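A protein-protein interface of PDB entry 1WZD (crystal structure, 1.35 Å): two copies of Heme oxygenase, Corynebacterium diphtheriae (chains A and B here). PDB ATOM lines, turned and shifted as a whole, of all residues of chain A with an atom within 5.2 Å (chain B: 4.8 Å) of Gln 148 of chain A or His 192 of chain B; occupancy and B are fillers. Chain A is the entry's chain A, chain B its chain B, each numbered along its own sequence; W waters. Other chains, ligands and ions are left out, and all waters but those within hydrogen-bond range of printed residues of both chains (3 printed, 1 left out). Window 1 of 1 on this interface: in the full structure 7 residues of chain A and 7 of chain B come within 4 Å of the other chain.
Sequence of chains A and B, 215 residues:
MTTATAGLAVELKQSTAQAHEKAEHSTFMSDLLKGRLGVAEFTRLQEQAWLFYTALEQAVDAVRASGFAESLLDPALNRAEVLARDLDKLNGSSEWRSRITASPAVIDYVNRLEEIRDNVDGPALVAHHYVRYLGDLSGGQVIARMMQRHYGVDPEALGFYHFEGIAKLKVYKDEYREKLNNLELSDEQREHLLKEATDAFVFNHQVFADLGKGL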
ATOM      1  N   ILE A 143       1.159 -22.621 -19.384  1.00  0.00           N
ATOM      2  CA  ILE A 143       0.580 -22.321 -20.690  1.00  0.00           C
ATOM      3  C   ILE A 143       0.225 -20.842 -20.794  1.00  0.00           C
ATOM      4  O   ILE A 143       0.551 -20.182 -21.785  1.00  0.00           O
ATOM      5  CB  ILE A 143      -0.631 -23.234 -20.989  1.00  0.00           C
ATOM      6  CG1 ILE A 143      -0.152 -24.693 -21.030  1.00  0.00           C
ATOM      7  CG2 ILE A 143      -1.300 -22.821 -22.304  1.00  0.00           C
ATOM      8  CD1 ILE A 143      -1.249 -25.733 -20.987  1.00  0.00           C
ATOM      9  N   ALA A 144      -0.415 -20.312 -19.760  1.00  0.00           N
ATOM     10  CA  ALA A 144      -0.754 -18.888 -19.726  1.00  0.00           C
ATOM     11  C   ALA A 144       0.482 -18.006 -19.880  1.00  0.00           C
ATOM     12  O   ALA A 144       0.443 -17.005 -20.607  1.00  0.00           O
ATOM     13  CB  ALA A 144      -1.496 -18.536 -18.447  1.00  0.00           C
ATOM     14  N   ARG A 145       1.573 -18.377 -19.205  1.00  0.00           N
ATOM     15  CA  ARG A 145       2.807 -17.603 -19.275  1.00  0.00           C
ATOM     16  C   ARG A 145       3.339 -17.629 -20.712  1.00  0.00           C
ATOM     17  O   ARG A 145       3.789 -16.618 -21.230  1.00  0.00           O
ATOM     18  CB  ARG A 145       3.851 -18.117 -18.262  1.00  0.00           C
ATOM     19  CG  ARG A 145       5.210 -17.370 -18.248  1.00  0.00           C
ATOM     20  CD  ARG A 145       5.071 -15.844 -18.148  1.00  0.00           C
ATOM     21  NE  ARG A 145       6.298 -15.179 -17.704  1.00  0.00           N
ATOM     22  CZ  ARG A 145       6.589 -14.925 -16.427  1.00  0.00           C
ATOM     23  NH1 ARG A 145       5.739 -15.269 -15.469  1.00  0.00           N
ATOM     24  NH2 ARG A 145       7.732 -14.324 -16.110  1.00  0.00           N
ATOM     25  N   MET A 146       3.244 -18.778 -21.367  1.00  0.00           N
ATOM     26  CA  MET A 146       3.681 -18.906 -22.746  1.00  0.00           C
ATOM     27  C   MET A 146       2.813 -18.094 -23.693  1.00  0.00           C
ATOM     28  O   MET A 146       3.321 -17.526 -24.657  1.00  0.00           O
ATOM     29  CB  MET A 146       3.755 -20.378 -23.167  1.00  0.00           C
ATOM     30  CG  MET A 146       4.788 -21.214 -22.391  1.00  0.00           C
ATOM     31  SD  MET A 146       6.471 -20.596 -22.579  1.00  0.00           S
ATOM     32  CE  MET A 146       6.556 -19.348 -21.346  1.00  0.00           C
ATOM     33  N   MET A 147       1.511 -18.009 -23.425  1.00  0.00           N
ATOM     34  CA  MET A 147       0.650 -17.225 -24.306  1.00  0.00           C
ATOM     35  C   MET A 147       0.973 -15.734 -24.211  1.00  0.00           C
ATOM     36  O   MET A 147       0.925 -15.020 -25.214  1.00  0.00           O
ATOM     37  CB  MET A 147      -0.835 -17.509 -24.056  1.00  0.00           C
ATOM     38  CG  MET A 147      -1.262 -18.974 -24.300  1.00  0.00           C
ATOM     39  SD  MET A 147      -0.774 -19.665 -25.895  1.00  0.00           S
ATOM     40  CE  MET A 147       0.851 -20.338 -25.534  1.00  0.00           C
ATOM     41  N   GLN A 148       1.304 -15.261 -23.016  1.00  0.00           N
ATOM     42  CA  GLN A 148       1.732 -13.875 -22.872  1.00  0.00           C
ATOM     43  C   GLN A 148       3.114 -13.651 -23.461  1.00  0.00           C
ATOM     44  O   GLN A 148       3.322 -12.676 -24.197  1.00  0.00           O
ATOM     45  CB  GLN A 148       1.736 -13.448 -21.412  1.00  0.00           C
ATOM     46  CG  GLN A 148       0.378 -13.484 -20.756  1.00  0.00           C
ATOM     47  CD  GLN A 148       0.357 -12.700 -19.471  1.00  0.00           C
ATOM     48  OE1 GLN A 148       0.141 -13.262 -18.395  1.00  0.00           O
ATOM     49  NE2 GLN A 148       0.588 -11.401 -19.571  1.00  0.00           N
ATOM     50  N   ARG A 149       4.040 -14.565 -23.178  1.00  0.00           N
ATOM     51  CA  ARG A 149       5.424 -14.411 -23.629  1.00  0.00           C
ATOM     52  C   ARG A 149       5.530 -14.425 -25.149  1.00  0.00           C
ATOM     53  O   ARG A 149       6.254 -13.614 -25.741  1.00  0.00           O
ATOM     54  CB  ARG A 149       6.319 -15.517 -23.064  1.00  0.00           C
ATOM     55  CG  ARG A 149       7.767 -15.395 -23.561  1.00  0.00           C
ATOM     56  CD  ARG A 149       8.657 -16.470 -22.988  1.00  0.00           C
ATOM     57  NE  ARG A 149       8.720 -16.378 -21.539  1.00  0.00           N
ATOM     58  CZ  ARG A 149       9.320 -17.275 -20.757  1.00  0.00           C
ATOM     59  NH1 ARG A 149       9.903 -18.340 -21.285  1.00  0.00           N
ATOM     60  NH2 ARG A 149       9.318 -17.096 -19.451  1.00  0.00           N
ATOM     61  N   HIS A 150       4.835 -15.364 -25.788  1.00  0.00           N
ATOM     62  CA  HIS A 150       4.979 -15.548 -27.226  1.00  0.00           C
ATOM     63  C   HIS A 150       4.008 -14.728 -28.053  1.00  0.00           C
ATOM     64  O   HIS A 150       4.373 -14.254 -29.135  1.00  0.00           O
ATOM     65  CB  HIS A 150       4.861 -17.021 -27.627  1.00  0.00           C
ATOM     66  CG  HIS A 150       5.982 -17.872 -27.130  1.00  0.00           C
ATOM     67  ND1 HIS A 150       7.306 -17.500 -27.242  1.00  0.00           N
ATOM     68  CD2 HIS A 150       5.978 -19.073 -26.508  1.00  0.00           C
ATOM     69  CE1 HIS A 150       8.068 -18.445 -26.723  1.00  0.00           C
ATOM     70  NE2 HIS A 150       7.287 -19.403 -26.260  1.00  0.00           N
ATOM     71  N   TYR A 151       2.780 -14.561 -27.561  1.00  0.00           N
ATOM     72  CA  TYR A 151       1.707 -14.042 -28.412  1.00  0.00           C
ATOM     73  C   TYR A 151       1.060 -12.780 -27.868  1.00  0.00           C
ATOM     74  O   TYR A 151       0.097 -12.283 -28.449  1.00  0.00           O
ATOM     75  CB  TYR A 151       0.666 -15.136 -28.684  1.00  0.00           C
ATOM     76  CG  TYR A 151       1.295 -16.417 -29.191  1.00  0.00           C
ATOM     77  CD1 TYR A 151       1.110 -17.632 -28.519  1.00  0.00           C
ATOM     78  CD2 TYR A 151       2.119 -16.405 -30.321  1.00  0.00           C
ATOM     79  CE1 TYR A 151       1.718 -18.798 -28.969  1.00  0.00           C
ATOM     80  CE2 TYR A 151       2.728 -17.557 -30.773  1.00  0.00           C
ATOM     81  CZ  TYR A 151       2.515 -18.756 -30.101  1.00  0.00           C
ATOM     82  OH  TYR A 151       3.108 -19.909 -30.545  1.00  0.00           O
ATOM     83  N   GLY A 152       1.591 -12.250 -26.771  1.00  0.00           N
ATOM     84  CA  GLY A 152       1.068 -11.005 -26.210  1.00  0.00           C
ATOM     85  C   GLY A 152      -0.396 -11.062 -25.808  1.00  0.00           C
ATOM     86  O   GLY A 152      -1.090 -10.044 -25.827  1.00  0.00           O
ATOM     87  N   VAL A 153      -0.881 -12.240 -25.424  1.00  0.00           N
ATOM     88  CA  VAL A 153      -2.295 -12.364 -25.057  1.00  0.00           C
ATOM     89  C   VAL A 153      -2.570 -11.576 -23.780  1.00  0.00           C
ATOM     90  O   VAL A 153      -1.818 -11.654 -22.813  1.00  0.00           O
ATOM     91  CB  VAL A 153      -2.734 -13.843 -24.888  1.00  0.00           C
ATOM     92  CG1 VAL A 153      -4.211 -13.930 -24.482  1.00  0.00           C
ATOM     93  CG2 VAL A 153      -2.494 -14.615 -26.185  1.00  0.00           C
ATOM     94  N   PRO A 155      -3.728 -10.771 -20.309  1.00  0.00           N
ATOM     95  CA  PRO A 155      -4.017 -11.673 -19.178  1.00  0.00           C
ATOM     96  C   PRO A 155      -5.501 -11.747 -18.812  1.00  0.00           C
ATOM     97  O   PRO A 155      -5.954 -12.764 -18.277  1.00  0.00           O
ATOM     98  CB  PRO A 155      -3.195 -11.086 -18.020  1.00  0.00           C
ATOM     99  CG  PRO A 155      -2.744  -9.740 -18.470  1.00  0.00           C
ATOM    100  CD  PRO A 155      -2.727  -9.743 -19.964  1.00  0.00           C
ATOM    101  N   LEU A 158      -7.104 -14.690 -20.395  1.00  0.00           N
ATOM    102  CA  LEU A 158      -6.585 -15.975 -19.944  1.00  0.00           C
ATOM    103  C   LEU A 158      -7.276 -16.407 -18.645  1.00  0.00           C
ATOM    104  O   LEU A 158      -6.695 -17.132 -17.821  1.00  0.00           O
ATOM    105  CB  LEU A 158      -5.067 -15.892 -19.755  1.00  0.00           C
ATOM    106  CG  LEU A 158      -4.251 -15.604 -21.023  1.00  0.00           C
ATOM    107  CD1 LEU A 158      -2.838 -15.194 -20.623  1.00  0.00           C
ATOM    108  CD2 LEU A 158      -4.235 -16.812 -21.959  1.00  0.00           C
ATOM    109  N   ASP B 121      -0.914  -5.144 -29.863  1.00  0.00           N
ATOM    110  CA  ASP B 121       0.134  -5.720 -29.028  1.00  0.00           C
ATOM    111  C   ASP B 121       1.262  -4.694 -28.911  1.00  0.00           C
ATOM    112  O   ASP B 121       2.196  -4.668 -29.730  1.00  0.00           O
ATOM    113  CB  ASP B 121       0.620  -7.028 -29.666  1.00  0.00           C
ATOM    114  CG  ASP B 121       1.606  -7.794 -28.799  1.00  0.00           C
ATOM    115  OD1 ASP B 121       2.134  -7.236 -27.815  1.00  0.00           O
ATOM    116  OD2 ASP B 121       1.872  -8.969 -29.149  1.00  0.00           O
ATOM    117  N   PRO B 123       3.861  -4.047 -26.628  1.00  0.00           N
ATOM    118  CA  PRO B 123       5.246  -4.525 -26.494  1.00  0.00           C
ATOM    119  C   PRO B 123       5.836  -5.122 -27.777  1.00  0.00           C
ATOM    120  O   PRO B 123       6.987  -4.832 -28.119  1.00  0.00           O
ATOM    121  CB  PRO B 123       5.145  -5.566 -25.376  1.00  0.00           C
ATOM    122  CG  PRO B 123       3.989  -5.057 -24.541  1.00  0.00           C
ATOM    123  CD  PRO B 123       2.994  -4.554 -25.547  1.00  0.00           C
ATOM    124  N   ALA B 124       5.063  -5.928 -28.501  1.00  0.00           N
ATOM    125  CA  ALA B 124       5.537  -6.454 -29.782  1.00  0.00           C
ATOM    126  C   ALA B 124       5.805  -5.336 -30.772  1.00  0.00           C
ATOM    127  O   ALA B 124       6.809  -5.363 -31.501  1.00  0.00           O
ATOM    128  CB  ALA B 124       4.549  -7.451 -30.356  1.00  0.00           C
ATOM    129  N   GLU B 188       6.039 -10.430 -18.166  1.00  0.00           N
ATOM    130  CA  GLU B 188       5.566 -11.110 -19.360  1.00  0.00           C
ATOM    131  C   GLU B 188       5.668 -10.218 -20.597  1.00  0.00           C
ATOM    132  O   GLU B 188       6.094 -10.683 -21.649  1.00  0.00           O
ATOM    133  CB  GLU B 188       4.127 -11.608 -19.166  1.00  0.00           C
ATOM    134  CG  GLU B 188       3.952 -12.639 -18.046  1.00  0.00           C
ATOM    135  CD  GLU B 188       3.577 -12.042 -16.703  1.00  0.00           C
ATOM    136  OE1 GLU B 188       2.952 -12.782 -15.912  1.00  0.00           O
ATOM    137  OE2 GLU B 188       3.888 -10.856 -16.427  1.00  0.00           O
ATOM    138  N   GLN B 189       5.273  -8.954 -20.467  1.00  0.00           N
ATOM    139  CA  GLN B 189       5.384  -7.999 -21.584  1.00  0.00           C
ATOM    140  C   GLN B 189       6.827  -7.784 -21.999  1.00  0.00           C
ATOM    141  O   GLN B 189       7.127  -7.704 -23.189  1.00  0.00           O
ATOM    142  CB  GLN B 189       4.776  -6.650 -21.223  1.00  0.00           C
ATOM    143  CG  GLN B 189       3.270  -6.625 -21.162  1.00  0.00           C
ATOM    144  CD  GLN B 189       2.763  -5.273 -20.714  1.00  0.00           C
ATOM    145  OE1 GLN B 189       3.269  -4.704 -19.751  1.00  0.00           O
ATOM    146  NE2 GLN B 189       1.764  -4.745 -21.418  1.00  0.00           N
ATOM    147  N   ARG B 190       7.722  -7.713 -21.015  1.00  0.00           N
ATOM    148  CA  ARG B 190       9.138  -7.518 -21.293  1.00  0.00           C
ATOM    149  C   ARG B 190       9.730  -8.738 -22.013  1.00  0.00           C
ATOM    150  O   ARG B 190      10.459  -8.598 -22.999  1.00  0.00           O
ATOM    151  CB  ARG B 190       9.898  -7.204 -19.998  1.00  0.00           C
ATOM    152  CG  ARG B 190      11.320  -6.697 -20.221  1.00  0.00           C
ATOM    153  CD  ARG B 190      11.989  -6.231 -18.919  1.00  0.00           C
ATOM    154  NE  ARG B 190      13.445  -6.151 -19.075  1.00  0.00           N
ATOM    155  CZ  ARG B 190      14.255  -5.316 -18.423  1.00  0.00           C
ATOM    156  NH1 ARG B 190      13.779  -4.442 -17.544  1.00  0.00           N
ATOM    157  NH2 ARG B 190      15.559  -5.357 -18.657  1.00  0.00           N
ATOM    158  N   GLU B 191       9.404  -9.938 -21.529  1.00  0.00           N
ATOM    159  CA  GLU B 191       9.823 -11.172 -22.211  1.00  0.00           C
ATOM    160  C   GLU B 191       9.314 -11.198 -23.661  1.00  0.00           C
ATOM    161  O   GLU B 191      10.034 -11.568 -24.587  1.00  0.00           O
ATOM    162  CB  GLU B 191       9.318 -12.411 -21.450  1.00  0.00           C
ATOM    163  CG  GLU B 191       9.970 -12.600 -20.091  1.00  0.00           C
ATOM    164  CD  GLU B 191       9.325 -13.686 -19.235  1.00  0.00           C
ATOM    165  OE1 GLU B 191       8.400 -14.397 -19.702  1.00  0.00           O
ATOM    166  OE2 GLU B 191       9.749 -13.830 -18.065  1.00  0.00           O
ATOM    167  N   HIS B 192       8.065 -10.786 -23.846  1.00  0.00           N
ATOM    168  CA  HIS B 192       7.457 -10.763 -25.166  1.00  0.00           C
ATOM    169  C   HIS B 192       8.147  -9.762 -26.100  1.00  0.00           C
ATOM    170  O   HIS B 192       8.410 -10.076 -27.266  1.00  0.00           O
ATOM    171  CB  HIS B 192       5.969 -10.468 -25.025  1.00  0.00           C
ATOM    172  CG  HIS B 192       5.214 -10.470 -26.317  1.00  0.00           C
ATOM    173  ND1 HIS B 192       5.279 -11.501 -27.232  1.00  0.00           N
ATOM    174  CD2 HIS B 192       4.326  -9.578 -26.814  1.00  0.00           C
ATOM    175  CE1 HIS B 192       4.483 -11.229 -28.251  1.00  0.00           C
ATOM    176  NE2 HIS B 192       3.901 -10.065 -28.027  1.00  0.00           N
ATOM    177  N   LEU B 193       8.450  -8.572 -25.581  1.00  0.00           N
ATOM    178  CA  LEU B 193       9.159  -7.560 -26.358  1.00  0.00           C
ATOM    179  C   LEU B 193      10.510  -8.103 -26.839  1.00  0.00           C
ATOM    180  O   LEU B 193      10.865  -7.974 -28.018  1.00  0.00           O
ATOM    181  CB  LEU B 193       9.326  -6.296 -25.511  1.00  0.00           C
ATOM    182  CG  LEU B 193       9.798  -5.014 -26.208  1.00  0.00           C
ATOM    183  CD1 LEU B 193       9.377  -3.805 -25.389  1.00  0.00           C
ATOM    184  CD2 LEU B 193      11.318  -5.020 -26.438  1.00  0.00           C
ATOM    185  N   LEU B 194      11.240  -8.740 -25.924  1.00  0.00           N
ATOM    186  CA  LEU B 194      12.540  -9.327 -26.273  1.00  0.00           C
ATOM    187  C   LEU B 194      12.418 -10.430 -27.318  1.00  0.00           C
ATOM    188  O   LEU B 194      13.167 -10.430 -28.296  1.00  0.00           O
ATOM    189  CB  LEU B 194      13.282  -9.826 -25.031  1.00  0.00           C
ATOM    190  CG  LEU B 194      13.676  -8.734 -24.043  1.00  0.00           C
ATOM    191  CD1 LEU B 194      14.134  -9.344 -22.723  1.00  0.00           C
ATOM    192  CD2 LEU B 194      14.757  -7.832 -24.615  1.00  0.00           C
ATOM    193  N   LYS B 195      11.461 -11.337 -27.116  1.00  0.00           N
ATOM    194  CA  LYS B 195      11.166 -12.417 -28.073  1.00  0.00           C
ATOM    195  C   LYS B 195      10.927 -11.810 -29.453  1.00  0.00           C
ATOM    196  O   LYS B 195      11.569 -12.183 -30.433  1.00  0.00           O
ATOM    197  CB  LYS B 195       9.934 -13.235 -27.610  1.00  0.00           C
ATOM    198  CG  LYS B 195       9.611 -14.519 -28.413  1.00  0.00           C
ATOM    199  CD  LYS B 195       8.560 -14.320 -29.524  1.00  0.00           C
ATOM    200  CE  LYS B 195       8.052 -15.672 -30.040  1.00  0.00           C
ATOM    201  NZ  LYS B 195       7.385 -15.583 -31.391  1.00  0.00           N
ATOM    202  N   GLU B 196      10.010 -10.849 -29.510  1.00  0.00           N
ATOM    203  CA  GLU B 196       9.623 -10.241 -30.769  1.00  0.00           C
ATOM    204  C   GLU B 196      10.764  -9.514 -31.483  1.00  0.00           C
ATOM    205  O   GLU B 196      10.827  -9.523 -32.713  1.00  0.00           O
ATOM    206  CB  GLU B 196       8.461  -9.284 -30.546  1.00  0.00           C
ATOM    207  CG  GLU B 196       7.762  -8.938 -31.819  1.00  0.00           C
ATOM    208  CD  GLU B 196       6.956 -10.100 -32.368  1.00  0.00           C
ATOM    209  OE1 GLU B 196       6.880 -10.227 -33.579  1.00  0.00           O
ATOM    210  OE2 GLU B 196       6.413 -10.873 -31.572  1.00  0.00           O
HETATM  211  O   HOH W   1       0.073 -11.650 -15.874  1.00  0.00           O
HETATM  212  O   HOH W   2       0.240 -10.087 -30.882  1.00  0.00           O
HETATM  213  O   HOH W   3       5.034 -14.078 -31.696  1.00  0.00           O
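Water W2 bridges the side-chain carboxylate (OD2) of Asp 121 of chain B and the backbone carbonyl oxygen (O) of Tyr 151 of chain A.
Water W3 lies within hydrogen-bond range of O of His 150 of chain A, NZ of Lys 195 of chain B and OE2 of Glu 196 of chain B.
Water W1 lies within hydrogen-bond range of the side-chain amide oxygen of Gln 148 of chain A and the side-chain carboxylate of Glu 188 of chain B.
The backbone NH (N) of Gly 152 of chain A sits close to a ring nitrogen (NE2) of His 192 of chain B, 3.4 Å away.
OE1 of Glu 191 of chain B lies within salt-bridge range of NE of Arg 149 of chain A, at 2.7 Å.
NH1 of Arg 145 of chain A lies within salt-bridge range of OE1 of Glu 188 of chain B (3.8 Å).
The guanidinium group (NH2) of Arg 145 of chain A is in salt-bridge range of the side-chain carboxylate (OE2) of Glu 191 of chain B, 2.9 Å away.
A ring nitrogen (ND1) of His 192 of chain B lies close to the backbone carbonyl oxygen of His 150 of chain A, at 3.5 Å.
The backbone carbonyl oxygen (O) of Arg 149 of chain A sits at hydrogen-bond distance from a ring nitrogen (ND1) of His 192 of chain B (2.8 Å).
Of the 13 printed residues of chain A, 6 touch a printed residue of chain B.
Printed residues of chain A that touch a printed residue of chain B: Arg 145, Gln 148, Arg 149, His 150, Tyr 151 and Gly 152.
Hydrophobic or aromatic side chains of chain A within 4 Å of the printed part of chain B: His 150.
Hydrophobic or aromatic side chains of chain B that line the printed part of chain A: His 192.
Among the printed residues, Asp or Glu carboxylates within 4 Å of a Lys or Arg side-chain nitrogen of the other chain: Arg 145 of chain A with Glu 188 of chain B, Arg 145 of chain A with Glu 191 of chain B and Arg 149 of chain A with Glu 191 of chain B.
Among the printed residues, merely in contact across the chains: Gln 148 of chain A with Glu 188 of chain B (3.6 Å), Gln 148 of chain A with His 192 of chain B (3.5 Å), His 150 of chain A with Lys 195 of chain B (3.4 Å), Tyr 151 of chain A with Asp 121 of chain B (3.8 Å), Tyr 151 of chain A with His 192 of chain B (3.8 Å) and Gly 152 of chain A with Asp 121 of chain B (3.7 Å).
No position is printed for both chains.
Of the 12 pairs that touch across the chains among the printed residues, none has its exchanged pair printed and touching as well.
Of chain B, only Glu 188 (3.6 Å) and His 192 (3.5 Å) come within 4 Å of Gln 148 of chain A.
Of the printed residues of chain B, His 150 of chain A touches His 192 (3.2 Å) and Lys 195 (3.4 Å).
Gln 189 of chain B touches none of the printed residues of chain A.
Printed residues of chain A within 4 Å of Glu 191 of chain B: Arg 145 (2.9 Å) and Arg 149 (2.7 Å).
Of chain A, only Gln 148, Arg 149, His 150, Tyr 151 and Gly 152 come within 4 Å of His 192 of chain B.
Glu 196 of chain B touches none of the printed residues of chain A.
The nearest printed residue of chain B that does not touch Gln 148 of chain A is Gln 189 of chain B (5.4 Å).
The nearest printed residue of chain B that does not touch Arg 149 of chain A is Lys 195 of chain B (4.1 Å).
The side-chain carboxylate (OD2) of Asp 121 of chain B lies within hydrogen-bond range of a ring nitrogen (NE2) of His 192 of chain B, at 2.6 Å.
The side-chain carboxylate (OD1) of Asp 121 of chain B lies within hydrogen-bond range of the backbone NH (N) of Ala 124 of chain B (3.3 Å).
The backbone NH (N) of Gly 152 of chain A lies within hydrogen-bond range of the backbone carbonyl oxygen (O) of Met 147 of chain A (3.2 Å).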
